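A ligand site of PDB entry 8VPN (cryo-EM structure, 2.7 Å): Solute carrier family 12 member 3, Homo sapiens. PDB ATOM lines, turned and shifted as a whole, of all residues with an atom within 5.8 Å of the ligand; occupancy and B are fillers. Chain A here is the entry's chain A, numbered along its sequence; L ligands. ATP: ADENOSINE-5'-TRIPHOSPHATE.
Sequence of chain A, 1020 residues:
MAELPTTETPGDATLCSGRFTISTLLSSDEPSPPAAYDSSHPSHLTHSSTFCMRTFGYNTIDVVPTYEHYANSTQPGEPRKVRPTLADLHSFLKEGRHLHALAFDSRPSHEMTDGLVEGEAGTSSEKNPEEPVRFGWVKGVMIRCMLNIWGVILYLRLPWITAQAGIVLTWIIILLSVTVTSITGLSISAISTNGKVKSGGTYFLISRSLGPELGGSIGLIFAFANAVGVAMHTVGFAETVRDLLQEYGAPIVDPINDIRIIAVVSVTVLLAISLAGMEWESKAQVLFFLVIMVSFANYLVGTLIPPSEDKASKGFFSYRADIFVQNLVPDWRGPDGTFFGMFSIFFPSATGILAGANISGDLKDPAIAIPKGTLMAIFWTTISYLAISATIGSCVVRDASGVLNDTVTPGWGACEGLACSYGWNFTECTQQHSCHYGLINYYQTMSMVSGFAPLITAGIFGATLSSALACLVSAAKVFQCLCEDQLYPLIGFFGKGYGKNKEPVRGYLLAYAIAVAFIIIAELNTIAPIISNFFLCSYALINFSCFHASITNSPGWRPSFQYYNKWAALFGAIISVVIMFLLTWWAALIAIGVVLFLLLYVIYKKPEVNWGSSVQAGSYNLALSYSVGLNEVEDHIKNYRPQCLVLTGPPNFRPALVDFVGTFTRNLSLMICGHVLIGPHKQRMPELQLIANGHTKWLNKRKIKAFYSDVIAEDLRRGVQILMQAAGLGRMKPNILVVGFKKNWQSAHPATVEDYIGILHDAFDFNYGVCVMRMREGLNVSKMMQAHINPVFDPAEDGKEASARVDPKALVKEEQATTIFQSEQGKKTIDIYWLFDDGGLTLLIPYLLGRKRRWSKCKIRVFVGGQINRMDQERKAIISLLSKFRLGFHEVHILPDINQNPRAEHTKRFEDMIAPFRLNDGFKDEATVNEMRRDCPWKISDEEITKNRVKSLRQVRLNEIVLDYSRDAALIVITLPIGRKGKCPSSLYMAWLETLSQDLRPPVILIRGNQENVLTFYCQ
N of Thr 648 touches N3 of the ligand (3.8 Å). Gly 649 touches the ligand (N to C2, 3.5 Å). Gly 674 touches the ligand. His 675 touches the ligand (CA to N1, 3.8 Å). Phe 741 touches the ligand (O to O3B, 3.9 Å). CB of Lys 742 touches O2A of the ligand, 3.4 Å away. CB of Leu 779 touches O2G of the ligand, 3.6 Å away. CB of Asn 780 touches O1G of the ligand, at 3.3 Å. Within 4 Å of the ligand: Leu 647, Thr 648, Gly 649, Arg 654, Gly 674, His 675, Val 676, Gly 740, Phe 741, Lys 742, Leu 779 and Asn 780.
O of Leu 647 is in hydrogen-bond range of O2' of the ligand, 2.5 Å away. N6 of the ligand sits at hydrogen-bond distance from O of Val 676 (3.2 Å). O of Gly 740 lies close to O3' of the ligand. N of Gly 740 sits close to O3' of the ligand, at 3.4 Å. The guanidinium group (NH2) of Arg 654 lies within salt-bridge range of an oxygen (O1G) of the ligand (3.2 Å). N of Val 676 lies within hydrogen-bond range of N1 of the ligand (3.4 Å).
N of Leu 647 lies within hydrogen-bond range of O of Val 738 (3.0 Å). NH1 of Arg 654 lies within hydrogen-bond range of O of Thr 648, at 3.2 Å. O of Gly 740 sits at hydrogen-bond distance from OH of Tyr 756 (2.8 Å). The backbone NH of Gly 649 sits at hydrogen-bond distance from the backbone carbonyl oxygen of Gly 674, at 3.0 Å. N of Thr 648 lies within hydrogen-bond range of O of Gly 674.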
ATOM      1  N   LEU A 647      16.564   5.916 -23.904  1.00  0.00           N
ATOM      2  CA  LEU A 647      15.995   7.265 -23.981  1.00  0.00           C
ATOM      3  C   LEU A 647      15.606   7.697 -22.571  1.00  0.00           C
ATOM      4  O   LEU A 647      14.591   7.249 -22.036  1.00  0.00           O
ATOM      5  CB  LEU A 647      14.798   7.302 -24.920  1.00  0.00           C
ATOM      6  CG  LEU A 647      15.084   7.014 -26.398  1.00  0.00           C
ATOM      7  CD1 LEU A 647      13.955   6.200 -26.989  1.00  0.00           C
ATOM      8  CD2 LEU A 647      15.307   8.293 -27.171  1.00  0.00           C
ATOM      9  N   THR A 648      16.403   8.579 -21.975  1.00  0.00           N
ATOM     10  CA  THR A 648      16.207   8.940 -20.579  1.00  0.00           C
ATOM     11  C   THR A 648      16.131  10.445 -20.328  1.00  0.00           C
ATOM     12  O   THR A 648      15.924  10.838 -19.172  1.00  0.00           O
ATOM     13  CB  THR A 648      17.328   8.360 -19.704  1.00  0.00           C
ATOM     14  OG1 THR A 648      18.591   8.873 -20.150  1.00  0.00           O
ATOM     15  CG2 THR A 648      17.362   6.853 -19.822  1.00  0.00           C
ATOM     16  N   GLY A 649      16.279  11.288 -21.341  1.00  0.00           N
ATOM     17  CA  GLY A 649      16.339  12.718 -21.128  1.00  0.00           C
ATOM     18  C   GLY A 649      17.438  13.056 -20.132  1.00  0.00           C
ATOM     19  O   GLY A 649      18.504  12.450 -20.122  1.00  0.00           O
ATOM     20  N   PRO A 650      17.183  14.033 -19.269  1.00  0.00           N
ATOM     21  CA  PRO A 650      18.128  14.309 -18.184  1.00  0.00           C
ATOM     22  C   PRO A 650      18.334  13.073 -17.332  1.00  0.00           C
ATOM     23  O   PRO A 650      17.366  12.469 -16.848  1.00  0.00           O
ATOM     24  CB  PRO A 650      17.429  15.426 -17.386  1.00  0.00           C
ATOM     25  CG  PRO A 650      16.479  16.046 -18.341  1.00  0.00           C
ATOM     26  CD  PRO A 650      16.041  14.957 -19.268  1.00  0.00           C
ATOM     27  N   ARG A 654      14.774  10.377 -14.573  1.00  0.00           N
ATOM     28  CA  ARG A 654      14.285   9.001 -14.493  1.00  0.00           C
ATOM     29  C   ARG A 654      15.438   8.079 -14.153  1.00  0.00           C
ATOM     30  O   ARG A 654      16.056   7.491 -15.050  1.00  0.00           O
ATOM     31  CB  ARG A 654      13.628   8.578 -15.807  1.00  0.00           C
ATOM     32  CG  ARG A 654      12.559   9.537 -16.314  1.00  0.00           C
ATOM     33  CD  ARG A 654      12.414   9.433 -17.814  1.00  0.00           C
ATOM     34  NE  ARG A 654      11.400  10.346 -18.338  1.00  0.00           N
ATOM     35  CZ  ARG A 654      11.660  11.471 -18.989  1.00  0.00           C
ATOM     36  NH1 ARG A 654      12.907  11.867 -19.202  1.00  0.00           N
ATOM     37  NH2 ARG A 654      10.657  12.208 -19.438  1.00  0.00           N
ATOM     38  N   LEU A 657      15.286   3.710 -14.776  1.00  0.00           N
ATOM     39  CA  LEU A 657      15.682   3.126 -16.044  1.00  0.00           C
ATOM     40  C   LEU A 657      17.200   2.979 -16.125  1.00  0.00           C
ATOM     41  O   LEU A 657      17.710   1.932 -16.552  1.00  0.00           O
ATOM     42  CB  LEU A 657      15.155   3.999 -17.196  1.00  0.00           C
ATOM     43  CG  LEU A 657      14.811   3.315 -18.519  1.00  0.00           C
ATOM     44  CD1 LEU A 657      13.892   2.129 -18.282  1.00  0.00           C
ATOM     45  CD2 LEU A 657      14.154   4.296 -19.478  1.00  0.00           C
ATOM     46  N   GLY A 674      20.446   8.897 -23.948  1.00  0.00           N
ATOM     47  CA  GLY A 674      20.033   9.882 -24.930  1.00  0.00           C
ATOM     48  C   GLY A 674      19.228  10.995 -24.305  1.00  0.00           C
ATOM     49  O   GLY A 674      18.561  10.809 -23.285  1.00  0.00           O
ATOM     50  N   HIS A 675      19.282  12.180 -24.923  1.00  0.00           N
ATOM     51  CA  HIS A 675      18.542  13.349 -24.451  1.00  0.00           C
ATOM     52  C   HIS A 675      18.321  14.271 -25.624  1.00  0.00           C
ATOM     53  O   HIS A 675      19.280  14.681 -26.285  1.00  0.00           O
ATOM     54  CB  HIS A 675      19.301  14.048 -23.318  1.00  0.00           C
ATOM     55  CG  HIS A 675      18.621  15.286 -22.815  1.00  0.00           C
ATOM     56  ND1 HIS A 675      19.280  16.221 -22.051  1.00  0.00           N
ATOM     57  CD2 HIS A 675      17.359  15.745 -22.972  1.00  0.00           C
ATOM     58  CE1 HIS A 675      18.444  17.199 -21.748  1.00  0.00           C
ATOM     59  NE2 HIS A 675      17.271  16.936 -22.292  1.00  0.00           N
ATOM     60  N   VAL A 676      17.063  14.608 -25.908  1.00  0.00           N
ATOM     61  CA  VAL A 676      16.698  15.413 -27.054  1.00  0.00           C
ATOM     62  C   VAL A 676      16.207  16.765 -26.560  1.00  0.00           C
ATOM     63  O   VAL A 676      15.188  16.849 -25.862  1.00  0.00           O
ATOM     64  CB  VAL A 676      15.628  14.724 -27.916  1.00  0.00           C
ATOM     65  CG1 VAL A 676      15.173  15.645 -29.035  1.00  0.00           C
ATOM     66  CG2 VAL A 676      16.175  13.431 -28.497  1.00  0.00           C
ATOM     67  N   LEU A 677      16.921  17.829 -26.923  1.00  0.00           N
ATOM     68  CA  LEU A 677      16.518  19.193 -26.662  1.00  0.00           C
ATOM     69  C   LEU A 677      15.911  19.766 -27.926  1.00  0.00           C
ATOM     70  O   LEU A 677      16.511  19.660 -29.005  1.00  0.00           O
ATOM     71  CB  LEU A 677      17.717  20.047 -26.219  1.00  0.00           C
ATOM     72  CG  LEU A 677      18.638  19.426 -25.175  1.00  0.00           C
ATOM     73  CD1 LEU A 677      20.048  19.958 -25.353  1.00  0.00           C
ATOM     74  CD2 LEU A 677      18.132  19.707 -23.784  1.00  0.00           C
ATOM     75  N   LEU A 716      10.716  14.963 -30.769  1.00  0.00           N
ATOM     76  CA  LEU A 716      11.421  13.818 -30.199  1.00  0.00           C
ATOM     77  C   LEU A 716      11.769  12.774 -31.251  1.00  0.00           C
ATOM     78  O   LEU A 716      12.868  12.201 -31.222  1.00  0.00           O
ATOM     79  CB  LEU A 716      10.563  13.195 -29.095  1.00  0.00           C
ATOM     80  CG  LEU A 716      10.839  11.742 -28.702  1.00  0.00           C
ATOM     81  CD1 LEU A 716      12.233  11.575 -28.110  1.00  0.00           C
ATOM     82  CD2 LEU A 716       9.795  11.257 -27.722  1.00  0.00           C
ATOM     83  N   VAL A 720      15.518  11.160 -31.975  1.00  0.00           N
ATOM     84  CA  VAL A 720      15.761   9.730 -31.820  1.00  0.00           C
ATOM     85  C   VAL A 720      16.292   9.140 -33.115  1.00  0.00           C
ATOM     86  O   VAL A 720      17.190   8.285 -33.105  1.00  0.00           O
ATOM     87  CB  VAL A 720      14.490   9.012 -31.350  1.00  0.00           C
ATOM     88  CG1 VAL A 720      14.647   7.507 -31.498  1.00  0.00           C
ATOM     89  CG2 VAL A 720      14.164   9.392 -29.917  1.00  0.00           C
ATOM     90  N   VAL A 738      15.872   1.154 -25.563  1.00  0.00           N
ATOM     91  CA  VAL A 738      15.129   0.999 -24.310  1.00  0.00           C
ATOM     92  C   VAL A 738      14.406   2.303 -24.010  1.00  0.00           C
ATOM     93  O   VAL A 738      15.038   3.348 -23.834  1.00  0.00           O
ATOM     94  CB  VAL A 738      16.056   0.603 -23.154  1.00  0.00           C
ATOM     95  CG1 VAL A 738      15.238   0.101 -21.987  1.00  0.00           C
ATOM     96  CG2 VAL A 738      17.031  -0.475 -23.608  1.00  0.00           C
ATOM     97  N   VAL A 739      13.078   2.216 -23.903  1.00  0.00           N
ATOM     98  CA  VAL A 739      12.214   3.369 -23.713  1.00  0.00           C
ATOM     99  C   VAL A 739      11.205   3.079 -22.608  1.00  0.00           C
ATOM    100  O   VAL A 739      10.890   1.917 -22.310  1.00  0.00           O
ATOM    101  CB  VAL A 739      11.492   3.768 -25.024  1.00  0.00           C
ATOM    102  CG1 VAL A 739      10.601   2.640 -25.488  1.00  0.00           C
ATOM    103  CG2 VAL A 739      10.691   5.039 -24.844  1.00  0.00           C
ATOM    104  N   GLY A 740      10.684   4.140 -22.006  1.00  0.00           N
ATOM    105  CA  GLY A 740       9.719   4.037 -20.938  1.00  0.00           C
ATOM    106  C   GLY A 740       8.299   4.281 -21.395  1.00  0.00           C
ATOM    107  O   GLY A 740       8.058   4.828 -22.465  1.00  0.00           O
ATOM    108  N   PHE A 741       7.352   3.871 -20.551  1.00  0.00           N
ATOM    109  CA  PHE A 741       5.937   3.881 -20.888  1.00  0.00           C
ATOM    110  C   PHE A 741       5.339   5.278 -20.690  1.00  0.00           C
ATOM    111  O   PHE A 741       5.604   5.941 -19.689  1.00  0.00           O
ATOM    112  CB  PHE A 741       5.188   2.865 -20.030  1.00  0.00           C
ATOM    113  CG  PHE A 741       3.818   2.517 -20.532  1.00  0.00           C
ATOM    114  CD1 PHE A 741       3.650   1.501 -21.453  1.00  0.00           C
ATOM    115  CD2 PHE A 741       2.708   3.205 -20.083  1.00  0.00           C
ATOM    116  CE1 PHE A 741       2.387   1.178 -21.912  1.00  0.00           C
ATOM    117  CE2 PHE A 741       1.445   2.882 -20.542  1.00  0.00           C
ATOM    118  CZ  PHE A 741       1.294   1.866 -21.463  1.00  0.00           C
ATOM    119  N   LYS A 742       4.522   5.710 -21.648  1.00  0.00           N
ATOM    120  CA  LYS A 742       3.816   6.994 -21.528  1.00  0.00           C
ATOM    121  C   LYS A 742       2.440   6.731 -20.927  1.00  0.00           C
ATOM    122  O   LYS A 742       1.449   6.536 -21.636  1.00  0.00           O
ATOM    123  CB  LYS A 742       3.731   7.692 -22.880  1.00  0.00           C
ATOM    124  CG  LYS A 742       3.023   6.907 -23.962  1.00  0.00           C
ATOM    125  CD  LYS A 742       2.574   7.821 -25.086  1.00  0.00           C
ATOM    126  CE  LYS A 742       1.903   9.066 -24.540  1.00  0.00           C
ATOM    127  NZ  LYS A 742       1.600  10.041 -25.618  1.00  0.00           N
ATOM    128  N   LYS A 743       2.382   6.750 -19.597  1.00  0.00           N
ATOM    129  CA  LYS A 743       1.176   6.364 -18.870  1.00  0.00           C
ATOM    130  C   LYS A 743       0.024   7.358 -19.032  1.00  0.00           C
ATOM    131  O   LYS A 743      -1.099   7.021 -18.674  1.00  0.00           O
ATOM    132  CB  LYS A 743       1.496   6.191 -17.390  1.00  0.00           C
ATOM    133  CG  LYS A 743       2.037   7.444 -16.708  1.00  0.00           C
ATOM    134  CD  LYS A 743       1.418   7.647 -15.340  1.00  0.00           C
ATOM    135  CE  LYS A 743       2.034   8.832 -14.620  1.00  0.00           C
ATOM    136  NZ  LYS A 743       3.294   8.450 -13.925  1.00  0.00           N
ATOM    137  N   ASN A 744       0.281   8.554 -19.551  1.00  0.00           N
ATOM    138  CA  ASN A 744      -0.740   9.571 -19.699  1.00  0.00           C
ATOM    139  C   ASN A 744      -1.269   9.673 -21.127  1.00  0.00           C
ATOM    140  O   ASN A 744      -1.621  10.761 -21.583  1.00  0.00           O
ATOM    141  CB  ASN A 744      -0.206  10.925 -19.237  1.00  0.00           C
ATOM    142  CG  ASN A 744      -1.293  11.816 -18.667  1.00  0.00           C
ATOM    143  OD1 ASN A 744      -2.252  11.332 -18.076  1.00  0.00           O
ATOM    144  ND2 ASN A 744      -1.149  13.127 -18.858  1.00  0.00           N
ATOM    145  N   THR A 752       0.845  13.357 -30.063  1.00  0.00           N
ATOM    146  CA  THR A 752       1.922  12.903 -29.178  1.00  0.00           C
ATOM    147  C   THR A 752       2.012  11.384 -29.166  1.00  0.00           C
ATOM    148  O   THR A 752       3.099  10.816 -29.343  1.00  0.00           O
ATOM    149  CB  THR A 752       1.686  13.440 -27.768  1.00  0.00           C
ATOM    150  OG1 THR A 752       2.132  14.805 -27.703  1.00  0.00           O
ATOM    151  CG2 THR A 752       2.475  12.620 -26.764  1.00  0.00           C
ATOM    152  N   TYR A 756       4.950   8.814 -30.511  1.00  0.00           N
ATOM    153  CA  TYR A 756       5.461   7.709 -29.705  1.00  0.00           C
ATOM    154  C   TYR A 756       5.437   6.397 -30.498  1.00  0.00           C
ATOM    155  O   TYR A 756       6.446   5.683 -30.587  1.00  0.00           O
ATOM    156  CB  TYR A 756       4.646   7.590 -28.425  1.00  0.00           C
ATOM    157  CG  TYR A 756       5.161   6.603 -27.413  1.00  0.00           C
ATOM    158  CD1 TYR A 756       4.653   5.315 -27.344  1.00  0.00           C
ATOM    159  CD2 TYR A 756       6.148   6.972 -26.497  1.00  0.00           C
ATOM    160  CE1 TYR A 756       5.113   4.418 -26.415  1.00  0.00           C
ATOM    161  CE2 TYR A 756       6.607   6.076 -25.568  1.00  0.00           C
ATOM    162  CZ  TYR A 756       6.090   4.799 -25.527  1.00  0.00           C
ATOM    163  OH  TYR A 756       6.555   3.896 -24.603  1.00  0.00           O
ATOM    164  N   GLY A 778       5.255   5.587 -11.679  1.00  0.00           N
ATOM    165  CA  GLY A 778       5.750   6.493 -12.701  1.00  0.00           C
ATOM    166  C   GLY A 778       7.267   6.555 -12.657  1.00  0.00           C
ATOM    167  O   GLY A 778       7.910   6.296 -11.647  1.00  0.00           O
ATOM    168  N   LEU A 779       7.861   6.909 -13.798  1.00  0.00           N
ATOM    169  CA  LEU A 779       9.306   6.959 -13.913  1.00  0.00           C
ATOM    170  C   LEU A 779       9.892   8.334 -13.661  1.00  0.00           C
ATOM    171  O   LEU A 779      11.019   8.433 -13.171  1.00  0.00           O
ATOM    172  CB  LEU A 779       9.748   6.482 -15.302  1.00  0.00           C
ATOM    173  CG  LEU A 779       9.880   4.973 -15.519  1.00  0.00           C
ATOM    174  CD1 LEU A 779       9.959   4.644 -17.002  1.00  0.00           C
ATOM    175  CD2 LEU A 779      11.089   4.425 -14.779  1.00  0.00           C
ATOM    176  N   ASN A 780       9.163   9.402 -13.975  1.00  0.00           N
ATOM    177  CA  ASN A 780       9.678  10.756 -13.788  1.00  0.00           C
ATOM    178  C   ASN A 780       9.243  11.341 -12.446  1.00  0.00           C
ATOM    179  O   ASN A 780      10.073  11.752 -11.639  1.00  0.00           O
ATOM    180  CB  ASN A 780       9.230  11.665 -14.925  1.00  0.00           C
ATOM    181  CG  ASN A 780       9.927  13.024 -14.901  1.00  0.00           C
ATOM    182  OD1 ASN A 780      10.907  13.217 -14.184  1.00  0.00           O
ATOM    183  ND2 ASN A 780       9.424  13.960 -15.689  1.00  0.00           N
HETATM  184  PG  ATP L   1       7.369   9.704 -17.984  1.00  0.00           P
HETATM  185  O1G ATP L   1       8.075  11.010 -17.902  1.00  0.00           O
HETATM  186  O2G ATP L   1       8.391   8.459 -17.978  1.00  0.00           O
HETATM  187  O3G ATP L   1       6.145   9.576 -16.947  1.00  0.00           O
HETATM  188  PB  ATP L   1       5.503  10.726 -19.778  1.00  0.00           P
HETATM  189  O1B ATP L   1       6.132  12.198 -19.719  1.00  0.00           O
HETATM  190  O2B ATP L   1       4.315  10.378 -18.974  1.00  0.00           O
HETATM  191  O3B ATP L   1       6.663   9.673 -19.426  1.00  0.00           O
HETATM  192  PA  ATP L   1       6.190  10.820 -22.473  1.00  0.00           P
HETATM  193  O1A ATP L   1       6.543  12.367 -22.263  1.00  0.00           O
HETATM  194  O2A ATP L   1       5.637  10.362 -23.775  1.00  0.00           O
HETATM  195  O3A ATP L   1       5.180  10.370 -21.308  1.00  0.00           O
HETATM  196  O5' ATP L   1       7.521   9.992 -22.150  1.00  0.00           O
HETATM  197  C5' ATP L   1       7.597   8.602 -22.445  1.00  0.00           C
HETATM  198  C4' ATP L   1       9.044   8.171 -22.606  1.00  0.00           C
HETATM  199  O4' ATP L   1       9.717   8.983 -23.589  1.00  0.00           O
HETATM  200  C3' ATP L   1       9.831   8.309 -21.320  1.00  0.00           C
HETATM  201  O3' ATP L   1       9.869   7.089 -20.598  1.00  0.00           O
HETATM  202  C2' ATP L   1      11.204   8.736 -21.741  1.00  0.00           C
HETATM  203  O2' ATP L   1      12.140   7.662 -21.607  1.00  0.00           O
HETATM  204  C1' ATP L   1      11.091   9.163 -23.197  1.00  0.00           C
HETATM  205  N9  ATP L   1      11.507  10.583 -23.344  1.00  0.00           N
HETATM  206  C8  ATP L   1      10.757  11.646 -23.059  1.00  0.00           C
HETATM  207  N7  ATP L   1      11.474  12.761 -23.298  1.00  0.00           N
HETATM  208  C5  ATP L   1      12.687  12.384 -23.744  1.00  0.00           C
HETATM  209  C6  ATP L   1      13.822  13.072 -24.143  1.00  0.00           C
HETATM  210  N6  ATP L   1      13.812  14.516 -24.122  1.00  0.00           N
HETATM  211  N1  ATP L   1      14.907  12.382 -24.539  1.00  0.00           N
HETATM  212  C2  ATP L   1      14.903  11.052 -24.559  1.00  0.00           C
HETATM  213  N3  ATP L   1      13.820  10.360 -24.170  1.00  0.00           N
HETATM  214  C4  ATP L   1      12.708  10.997 -23.764  1.00  0.00           C
